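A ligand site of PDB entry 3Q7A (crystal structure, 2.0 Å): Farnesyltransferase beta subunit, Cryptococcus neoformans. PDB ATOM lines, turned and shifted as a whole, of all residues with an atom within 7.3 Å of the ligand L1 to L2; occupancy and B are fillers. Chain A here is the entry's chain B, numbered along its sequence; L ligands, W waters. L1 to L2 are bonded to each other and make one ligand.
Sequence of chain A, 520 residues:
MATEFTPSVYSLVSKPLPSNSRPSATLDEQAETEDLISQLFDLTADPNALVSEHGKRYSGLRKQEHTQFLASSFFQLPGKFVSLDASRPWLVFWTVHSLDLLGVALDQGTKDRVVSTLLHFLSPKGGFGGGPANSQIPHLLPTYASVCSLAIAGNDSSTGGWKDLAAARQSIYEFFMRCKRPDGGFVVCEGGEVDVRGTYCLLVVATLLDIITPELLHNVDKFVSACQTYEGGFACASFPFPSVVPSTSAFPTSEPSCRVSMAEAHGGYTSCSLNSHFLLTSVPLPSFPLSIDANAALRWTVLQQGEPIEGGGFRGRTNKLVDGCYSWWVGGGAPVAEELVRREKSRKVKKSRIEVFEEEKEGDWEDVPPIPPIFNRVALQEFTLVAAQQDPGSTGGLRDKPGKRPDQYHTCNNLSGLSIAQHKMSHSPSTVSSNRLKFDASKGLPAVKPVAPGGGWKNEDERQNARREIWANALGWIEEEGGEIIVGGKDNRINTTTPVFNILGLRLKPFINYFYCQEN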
ATOM      1  N   ALA A   2     -25.323  12.813   8.982  1.00  0.00           N
ATOM      2  CA  ALA A   2     -24.787  13.912   8.115  1.00  0.00           C
ATOM      3  C   ALA A   2     -23.283  13.776   7.884  1.00  0.00           C
ATOM      4  O   ALA A   2     -22.778  14.169   6.818  1.00  0.00           O
ATOM      5  CB  ALA A   2     -25.111  15.265   8.728  1.00  0.00           C
ATOM      6  N   THR A   3     -22.575  13.219   8.866  1.00  0.00           N
ATOM      7  CA  THR A   3     -21.119  13.082   8.800  1.00  0.00           C
ATOM      8  C   THR A   3     -20.646  11.625   8.653  1.00  0.00           C
ATOM      9  O   THR A   3     -19.462  11.338   8.800  1.00  0.00           O
ATOM     10  CB  THR A   3     -20.426  13.720  10.024  1.00  0.00           C
ATOM     11  OG1 THR A   3     -20.923  13.111  11.230  1.00  0.00           O
ATOM     12  CG2 THR A   3     -20.680  15.230  10.070  1.00  0.00           C
ATOM     13  N   THR A   6     -18.084  11.394   5.944  1.00  0.00           N
ATOM     14  CA  THR A   6     -17.050  12.439   6.006  1.00  0.00           C
ATOM     15  C   THR A   6     -16.234  12.312   7.304  1.00  0.00           C
ATOM     16  O   THR A   6     -16.412  13.114   8.227  1.00  0.00           O
ATOM     17  CB  THR A   6     -17.654  13.857   5.915  1.00  0.00           C
ATOM     18  OG1 THR A   6     -18.645  14.035   6.930  1.00  0.00           O
ATOM     19  CG2 THR A   6     -18.281  14.093   4.551  1.00  0.00           C
ATOM     20  N   ASP A  46      -8.442  18.670  18.510  1.00  0.00           N
ATOM     21  CA  ASP A  46      -9.490  18.214  17.600  1.00  0.00           C
ATOM     22  C   ASP A  46     -10.671  19.187  17.680  1.00  0.00           C
ATOM     23  O   ASP A  46     -11.239  19.373  18.759  1.00  0.00           O
ATOM     24  CB  ASP A  46      -9.914  16.790  18.009  1.00  0.00           C
ATOM     25  CG  ASP A  46     -10.952  16.180  17.074  1.00  0.00           C
ATOM     26  OD1 ASP A  46     -11.496  16.866  16.173  1.00  0.00           O
ATOM     27  OD2 ASP A  46     -11.237  14.974  17.244  1.00  0.00           O
ATOM     28  N   PRO A  47     -11.029  19.835  16.549  1.00  0.00           N
ATOM     29  CA  PRO A  47     -12.143  20.798  16.550  1.00  0.00           C
ATOM     30  C   PRO A  47     -13.491  20.169  16.921  1.00  0.00           C
ATOM     31  O   PRO A  47     -14.385  20.866  17.377  1.00  0.00           O
ATOM     32  CB  PRO A  47     -12.193  21.276  15.087  1.00  0.00           C
ATOM     33  CG  PRO A  47     -10.875  20.925  14.505  1.00  0.00           C
ATOM     34  CD  PRO A  47     -10.418  19.701  15.212  1.00  0.00           C
ATOM     35  N   ASN A  48     -13.604  18.859  16.721  1.00  0.00           N
ATOM     36  CA  ASN A  48     -14.856  18.132  16.977  1.00  0.00           C
ATOM     37  C   ASN A  48     -15.068  17.750  18.440  1.00  0.00           C
ATOM     38  O   ASN A  48     -16.199  17.492  18.850  1.00  0.00           O
ATOM     39  CB  ASN A  48     -14.923  16.888  16.085  1.00  0.00           C
ATOM     40  CG  ASN A  48     -14.766  17.204  14.614  1.00  0.00           C
ATOM     41  OD1 ASN A  48     -15.705  17.664  13.956  1.00  0.00           O
ATOM     42  ND2 ASN A  48     -13.574  16.969  14.077  1.00  0.00           N
ATOM     43  N   ALA A  49     -13.977  17.713  19.213  1.00  0.00           N
ATOM     44  CA  ALA A  49     -13.993  17.212  20.588  1.00  0.00           C
ATOM     45  C   ALA A  49     -14.749  18.114  21.563  1.00  0.00           C
ATOM     46  O   ALA A  49     -14.705  19.345  21.454  1.00  0.00           O
ATOM     47  CB  ALA A  49     -12.566  16.973  21.080  1.00  0.00           C
ATOM     48  N   LEU A  50     -15.442  17.485  22.524  1.00  0.00           N
ATOM     49  CA  LEU A  50     -16.109  18.193  23.616  1.00  0.00           C
ATOM     50  C   LEU A  50     -15.085  18.664  24.652  1.00  0.00           C
ATOM     51  O   LEU A  50     -15.052  19.839  25.010  1.00  0.00           O
ATOM     52  CB  LEU A  50     -17.161  17.309  24.288  1.00  0.00           C
ATOM     53  CG  LEU A  50     -18.525  17.148  23.625  1.00  0.00           C
ATOM     54  CD1 LEU A  50     -19.337  16.081  24.352  1.00  0.00           C
ATOM     55  CD2 LEU A  50     -19.300  18.468  23.570  1.00  0.00           C
ATOM     56  N   VAL A 378     -15.836  17.533   6.061  1.00  0.00           N
ATOM     57  CA  VAL A 378     -15.294  17.706   7.412  1.00  0.00           C
ATOM     58  C   VAL A 378     -13.784  17.932   7.368  1.00  0.00           C
ATOM     59  O   VAL A 378     -13.274  18.885   7.949  1.00  0.00           O
ATOM     60  CB  VAL A 378     -15.675  16.525   8.345  1.00  0.00           C
ATOM     61  CG1 VAL A 378     -14.862  16.553   9.635  1.00  0.00           C
ATOM     62  CG2 VAL A 378     -17.173  16.557   8.664  1.00  0.00           C
ATOM     63  N   GLN A 381     -12.689  21.412   6.118  1.00  0.00           N
ATOM     64  CA  GLN A 381     -12.856  22.428   7.151  1.00  0.00           C
ATOM     65  C   GLN A 381     -11.737  22.327   8.177  1.00  0.00           C
ATOM     66  O   GLN A 381     -11.206  23.340   8.642  1.00  0.00           O
ATOM     67  CB  GLN A 381     -14.222  22.319   7.821  1.00  0.00           C
ATOM     68  CG  GLN A 381     -15.393  22.586   6.874  1.00  0.00           C
ATOM     69  CD  GLN A 381     -16.738  22.464   7.548  1.00  0.00           C
ATOM     70  OE1 GLN A 381     -17.626  21.759   7.076  1.00  0.00           O
ATOM     71  NE2 GLN A 381     -16.913  23.168   8.663  1.00  0.00           N
ATOM     72  N   GLU A 382     -11.363  21.086   8.521  1.00  0.00           N
ATOM     73  CA  GLU A 382     -10.263  20.848   9.453  1.00  0.00           C
ATOM     74  C   GLU A 382      -8.935  21.362   8.908  1.00  0.00           C
ATOM     75  O   GLU A 382      -8.164  21.977   9.645  1.00  0.00           O
ATOM     76  CB  GLU A 382     -10.176  19.365   9.807  1.00  0.00           C
ATOM     77  CG  GLU A 382     -11.322  18.884  10.681  1.00  0.00           C
ATOM     78  CD  GLU A 382     -11.305  17.393  10.915  1.00  0.00           C
ATOM     79  OE1 GLU A 382     -10.861  16.646  10.013  1.00  0.00           O
ATOM     80  OE2 GLU A 382     -11.740  16.961  11.998  1.00  0.00           O
ATOM     81  N   GLN A 422     -18.808  24.003   4.294  1.00  0.00           N
ATOM     82  CA  GLN A 422     -19.764  24.233   5.370  1.00  0.00           C
ATOM     83  C   GLN A 422     -21.207  24.086   4.910  1.00  0.00           C
ATOM     84  O   GLN A 422     -22.050  23.556   5.633  1.00  0.00           O
ATOM     85  CB  GLN A 422     -19.570  25.624   5.981  1.00  0.00           C
ATOM     86  CG  GLN A 422     -18.420  25.735   6.962  1.00  0.00           C
ATOM     87  CD  GLN A 422     -18.365  27.103   7.636  1.00  0.00           C
ATOM     88  OE1 GLN A 422     -19.157  27.994   7.327  1.00  0.00           O
ATOM     89  NE2 GLN A 422     -17.426  27.268   8.565  1.00  0.00           N
ATOM     90  N   GLY A 482     -30.946  21.357   5.975  1.00  0.00           N
ATOM     91  CA  GLY A 482     -30.346  20.276   6.759  1.00  0.00           C
ATOM     92  C   GLY A 482     -28.986  19.823   6.260  1.00  0.00           C
ATOM     93  O   GLY A 482     -28.433  18.846   6.766  1.00  0.00           O
ATOM     94  N   GLY A 483     -28.435  20.521   5.268  1.00  0.00           N
ATOM     95  CA  GLY A 483     -27.155  20.151   4.671  1.00  0.00           C
ATOM     96  C   GLY A 483     -25.947  20.807   5.326  1.00  0.00           C
ATOM     97  O   GLY A 483     -24.806  20.545   4.937  1.00  0.00           O
ATOM     98  N   GLU A 484     -26.200  21.661   6.321  1.00  0.00           N
ATOM     99  CA  GLU A 484     -25.141  22.431   6.959  1.00  0.00           C
ATOM    100  C   GLU A 484     -24.286  21.565   7.893  1.00  0.00           C
ATOM    101  O   GLU A 484     -24.805  20.831   8.724  1.00  0.00           O
ATOM    102  CB  GLU A 484     -25.743  23.601   7.734  1.00  0.00           C
ATOM    103  CG  GLU A 484     -24.769  24.721   8.047  1.00  0.00           C
ATOM    104  CD  GLU A 484     -25.415  25.866   8.818  1.00  0.00           C
ATOM    105  OE1 GLU A 484     -25.336  27.016   8.338  1.00  0.00           O
ATOM    106  OE2 GLU A 484     -25.991  25.612   9.892  1.00  0.00           O
ATOM    107  N   ILE A 485     -22.960  21.654   7.723  1.00  0.00           N
ATOM    108  CA  ILE A 485     -22.015  21.021   8.648  1.00  0.00           C
ATOM    109  C   ILE A 485     -20.957  22.057   9.014  1.00  0.00           C
ATOM    110  O   ILE A 485     -20.082  22.370   8.204  1.00  0.00           O
ATOM    111  CB  ILE A 485     -21.321  19.757   8.053  1.00  0.00           C
ATOM    112  CG1 ILE A 485     -22.359  18.724   7.590  1.00  0.00           C
ATOM    113  CG2 ILE A 485     -20.379  19.121   9.086  1.00  0.00           C
ATOM    114  CD1 ILE A 485     -21.778  17.568   6.775  1.00  0.00           C
ATOM    115  N   ILE A 486     -21.054  22.596  10.229  1.00  0.00           N
ATOM    116  CA  ILE A 486     -20.078  23.562  10.718  1.00  0.00           C
ATOM    117  C   ILE A 486     -19.159  22.883  11.728  1.00  0.00           C
ATOM    118  O   ILE A 486     -19.507  22.744  12.912  1.00  0.00           O
ATOM    119  CB  ILE A 486     -20.738  24.825  11.332  1.00  0.00           C
ATOM    120  CG1 ILE A 486     -21.911  25.327  10.481  1.00  0.00           C
ATOM    121  CG2 ILE A 486     -19.690  25.915  11.577  1.00  0.00           C
ATOM    122  CD1 ILE A 486     -21.525  25.848   9.101  1.00  0.00           C
ATOM    123  N   VAL A 487     -17.986  22.469  11.256  1.00  0.00           N
ATOM    124  CA  VAL A 487     -16.985  21.807  12.102  1.00  0.00           C
ATOM    125  C   VAL A 487     -16.486  22.757  13.193  1.00  0.00           C
ATOM    126  O   VAL A 487     -16.101  23.884  12.903  1.00  0.00           O
ATOM    127  CB  VAL A 487     -15.807  21.262  11.248  1.00  0.00           C
ATOM    128  CG1 VAL A 487     -14.663  20.753  12.132  1.00  0.00           C
ATOM    129  CG2 VAL A 487     -16.289  20.158  10.305  1.00  0.00           C
ATOM    130  N   GLY A 488     -16.520  22.289  14.439  1.00  0.00           N
ATOM    131  CA  GLY A 488     -16.035  23.074  15.568  1.00  0.00           C
ATOM    132  C   GLY A 488     -17.072  23.962  16.225  1.00  0.00           C
ATOM    133  O   GLY A 488     -16.769  24.688  17.166  1.00  0.00           O
ATOM    134  N   GLY A 489     -18.302  23.913  15.716  1.00  0.00           N
ATOM    135  CA  GLY A 489     -19.402  24.677  16.297  1.00  0.00           C
ATOM    136  C   GLY A 489     -19.778  25.919  15.509  1.00  0.00           C
ATOM    137  O   GLY A 489     -19.017  26.389  14.665  1.00  0.00           O
ATOM    138  N   LYS A 490     -20.958  26.458  15.814  1.00  0.00           N
ATOM    139  CA  LYS A 490     -21.586  27.493  14.995  1.00  0.00           C
ATOM    140  C   LYS A 490     -20.832  28.826  14.933  1.00  0.00           C
ATOM    141  O   LYS A 490     -21.030  29.590  13.992  1.00  0.00           O
ATOM    142  CB  LYS A 490     -23.043  27.689  15.411  1.00  0.00           C
ATOM    143  CG  LYS A 490     -23.932  26.505  15.024  1.00  0.00           C
ATOM    144  CD  LYS A 490     -25.364  26.674  15.475  1.00  0.00           C
ATOM    145  CE  LYS A 490     -26.233  25.551  14.933  1.00  0.00           C
ATOM    146  NZ  LYS A 490     -27.665  25.742  15.305  1.00  0.00           N
ATOM    147  N   ASP A 491     -19.944  29.081  15.897  1.00  0.00           N
ATOM    148  CA  ASP A 491     -19.102  30.274  15.837  1.00  0.00           C
ATOM    149  C   ASP A 491     -18.112  30.265  14.666  1.00  0.00           C
ATOM    150  O   ASP A 491     -17.613  31.309  14.252  1.00  0.00           O
ATOM    151  CB  ASP A 491     -18.376  30.494  17.166  1.00  0.00           C
ATOM    152  CG  ASP A 491     -19.282  31.052  18.250  1.00  0.00           C
ATOM    153  OD1 ASP A 491     -20.164  31.884  17.936  1.00  0.00           O
ATOM    154  OD2 ASP A 491     -19.119  30.655  19.413  1.00  0.00           O
ATOM    155  N   ASN A 492     -17.840  29.077  14.133  1.00  0.00           N
ATOM    156  CA  ASN A 492     -17.009  28.932  12.935  1.00  0.00           C
ATOM    157  C   ASN A 492     -17.726  29.192  11.609  1.00  0.00           C
ATOM    158  O   ASN A 492     -17.085  29.230  10.552  1.00  0.00           O
ATOM    159  CB  ASN A 492     -16.365  27.546  12.893  1.00  0.00           C
ATOM    160  CG  ASN A 492     -15.253  27.391  13.910  1.00  0.00           C
ATOM    161  OD1 ASN A 492     -14.711  28.372  14.416  1.00  0.00           O
ATOM    162  ND2 ASN A 492     -14.900  26.142  14.210  1.00  0.00           N
ATOM    163  N   ARG A 493     -19.053  29.379  11.670  1.00  0.00           N
ATOM    164  CA  ARG A 493     -19.865  29.573  10.470  1.00  0.00           C
ATOM    165  C   ARG A 493     -19.522  30.847   9.710  1.00  0.00           C
ATOM    166  O   ARG A 493     -19.506  31.943  10.278  1.00  0.00           O
ATOM    167  CB  ARG A 493     -21.373  29.579  10.805  1.00  0.00           C
ATOM    168  CG  ARG A 493     -22.271  29.610   9.567  1.00  0.00           C
ATOM    169  CD  ARG A 493     -23.670  30.113   9.871  1.00  0.00           C
ATOM    170  NE  ARG A 493     -24.512  30.114   8.675  1.00  0.00           N
ATOM    171  CZ  ARG A 493     -24.663  31.149   7.845  1.00  0.00           C
ATOM    172  NH1 ARG A 493     -24.030  32.300   8.054  1.00  0.00           N
ATOM    173  NH2 ARG A 493     -25.445  31.038   6.781  1.00  0.00           N
HETATM  174  C1  LIG L   1     -21.447  19.605  15.822  1.00  0.00           C
HETATM  175  C2  LIG L   1     -20.409  19.459  16.951  1.00  0.00           C
HETATM  176  C3  LIG L   1     -19.007  19.832  16.472  1.00  0.00           C
HETATM  177  C4  LIG L   1     -18.636  19.088  15.169  1.00  0.00           C
HETATM  178  C5  LIG L   1     -19.740  19.276  14.121  1.00  0.00           C
HETATM  179  C6  LIG L   1     -19.434  18.520  12.810  1.00  0.00           C
HETATM  180  O1  LIG L   1     -20.780  20.298  18.053  1.00  0.00           O
HETATM  181  O2  LIG L   1     -18.048  19.535  17.490  1.00  0.00           O
HETATM  182  O3  LIG L   1     -17.389  19.601  14.687  1.00  0.00           O
HETATM  183  O4  LIG L   1     -21.034  18.866  14.648  1.00  0.00           O
HETATM  184  O5  LIG L   1     -19.776  17.139  12.950  1.00  0.00           O
HETATM  185  C1  LG2 L   2     -23.540  22.028  16.586  1.00  0.00           C
HETATM  186  C2  LG2 L   2     -22.979  21.460  15.279  1.00  0.00           C
HETATM  187  C3  LG2 L   2     -22.976  22.520  14.155  1.00  0.00           C
HETATM  188  C4  LG2 L   2     -23.032  21.627  12.930  1.00  0.00           C
HETATM  189  C5  LG2 L   2     -24.127  20.659  13.369  1.00  0.00           C
HETATM  190  C6  LG2 L   2     -24.148  19.359  12.535  1.00  0.00           C
HETATM  191  O1  LG2 L   2     -24.915  22.394  16.414  1.00  0.00           O
HETATM  192  O2  LG2 L   2     -21.620  21.020  15.516  1.00  0.00           O
HETATM  193  O3  LG2 L   2     -21.769  23.286  14.183  1.00  0.00           O
HETATM  194  O4  LG2 L   2     -23.445  22.352  11.777  1.00  0.00           O
HETATM  195  O5  LG2 L   2     -23.821  20.383  14.772  1.00  0.00           O
HETATM  196  O6  LG2 L   2     -22.869  18.716  12.620  1.00  0.00           O
HETATM  197  O1  LG3 L   3     -23.798  24.851  19.817  1.00  0.00           O
HETATM  198  O2  LG3 L   3     -22.229  25.196  18.041  1.00  0.00           O
HETATM  199  O3  LG3 L   3     -20.746  27.926  18.764  1.00  0.00           O
HETATM  200  O4  LG3 L   3     -23.618  27.031  18.732  1.00  0.00           O
HETATM  201  C1  LG3 L   3     -15.606  30.341  22.928  1.00  0.00           C
HETATM  202  C2  LG3 L   3     -16.835  29.690  23.576  1.00  0.00           C
HETATM  203  C3  LG3 L   3     -15.059  29.480  21.775  1.00  0.00           C
HETATM  204  C4  LG3 L   3     -17.920  29.432  22.515  1.00  0.00           C
HETATM  205  C5  LG3 L   3     -16.152  29.175  20.727  1.00  0.00           C
HETATM  206  C6  LG3 L   3     -19.354  27.315  20.671  1.00  0.00           C
HETATM  207  C7  LG3 L   3     -21.564  26.255  20.393  1.00  0.00           C
HETATM  208  N1  LG3 L   3     -18.444  28.411  20.323  1.00  0.00           N
HETATM  209  C8  LG3 L   3     -20.768  27.545  20.154  1.00  0.00           C
HETATM  210  C9  LG3 L   3     -17.408  28.546  21.364  1.00  0.00           C
HETATM  211  S1  LG3 L   3     -22.851  25.823  19.174  1.00  0.00           S
HETATM  212  O   HOH W   1     -17.183  21.704  18.798  1.00  0.00           O
HETATM  213  O   HOH W   2     -20.502  22.959  19.018  1.00  0.00           O
HETATM  214  O   HOH W   3     -23.186  18.974  18.931  1.00  0.00           O
HETATM  215  O   HOH W   4     -25.452  24.016  11.887  1.00  0.00           O
HETATM  216  O   HOH W   5     -25.792  23.443  18.693  1.00  0.00           O
HETATM  217  O   HOH W   6     -17.223  16.028  12.506  1.00  0.00           O
HETATM  218  O   HOH W   7     -26.839  20.741  15.522  1.00  0.00           O
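The backbone NH (N) of Asp 491 is in hydrogen-bond range of an oxygen (O3) of LG3 L3 (3.2 Å).
N of Gly 488 lies within hydrogen-bond range of O3 of LIG L1, at 2.8 Å.
N1 of LG3 L3 is in salt-bridge range of OD2 of Asp 491 (2.5 Å).
N of Ile 486 sits at hydrogen-bond distance from O4 of LG2 L2 (2.9 Å).
An oxygen (O2) of LG3 L3 is in hydrogen-bond range of the backbone NH (N) of Lys 490 (2.9 Å).
O3 of LIG L1 sits at hydrogen-bond distance from OD1 of Asn 48, at 2.7 Å.
The backbone carbonyl oxygen (O) of Asn 48 is in hydrogen-bond range of an oxygen (O2) of LIG L1, at 3.1 Å.
The backbone carbonyl oxygen of Ile 486 is in hydrogen-bond range of an oxygen (O3) of LG2 L2, at 2.7 Å.
Water W4 lies within hydrogen-bond range of O4 of LG2 L2 (2.6 Å) and OE2 of Glu 484 (2.6 Å).
Water W5 lies within hydrogen-bond range of O1 of LG2 L2 (2.7 Å) and O1 of LG3 L3 (2.7 Å).
Water W1 lies within hydrogen-bond range of an oxygen (O2) of LIG L1 (2.7 Å), the backbone carbonyl oxygen of Pro 47 (3.2 Å) and the backbone carbonyl oxygen of Gly 488 (3.4 Å).
Water W6 lies within hydrogen-bond range of OD1 of Asn 48 and O5 of LIG L1.
Water W2 lies within hydrogen-bond range of an oxygen (O1) of LIG L1 (2.8 Å) and an oxygen (O2) of LG3 L3 (3.0 Å).
OE2 of Glu 382 sits at hydrogen-bond distance from ND2 of Asn 48 (2.8 Å).
OE1 of Gln 381 sits close to O of Ile 485, 2.8 Å away.
OE1 of Glu 484 lies within salt-bridge range of NE of Arg 493.
OG1 of Thr 6 lies close to O of Thr 3 (3.4 Å).
The backbone NH of Val 487 lies close to the side-chain amide nitrogen of Gln 381 (2.9 Å).
ND2 of Asn 492 is in hydrogen-bond range of O of Val 487 (2.9 Å).
OD1 of Asp 46 sits at hydrogen-bond distance from N of Asn 48 (3.0 Å).
N of Ile 485 is in hydrogen-bond range of O of Gln 422 (3.0 Å).
Residues that only touch the ligand L1 to L2: Val 487, Gly 489, Thr 3, Lys 490, Glu 484, Ile 485 and Pro 47.
Within 4 Å of the ligand L1 to L2: Thr 3, Pro 47, Asn 48, Glu 484, Ile 485, Ile 486, Val 487, Gly 488, Gly 489 and Lys 490.
Along chain A the residues within 4 Å of the ligand L1 to L2 span positions 3 to 490.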
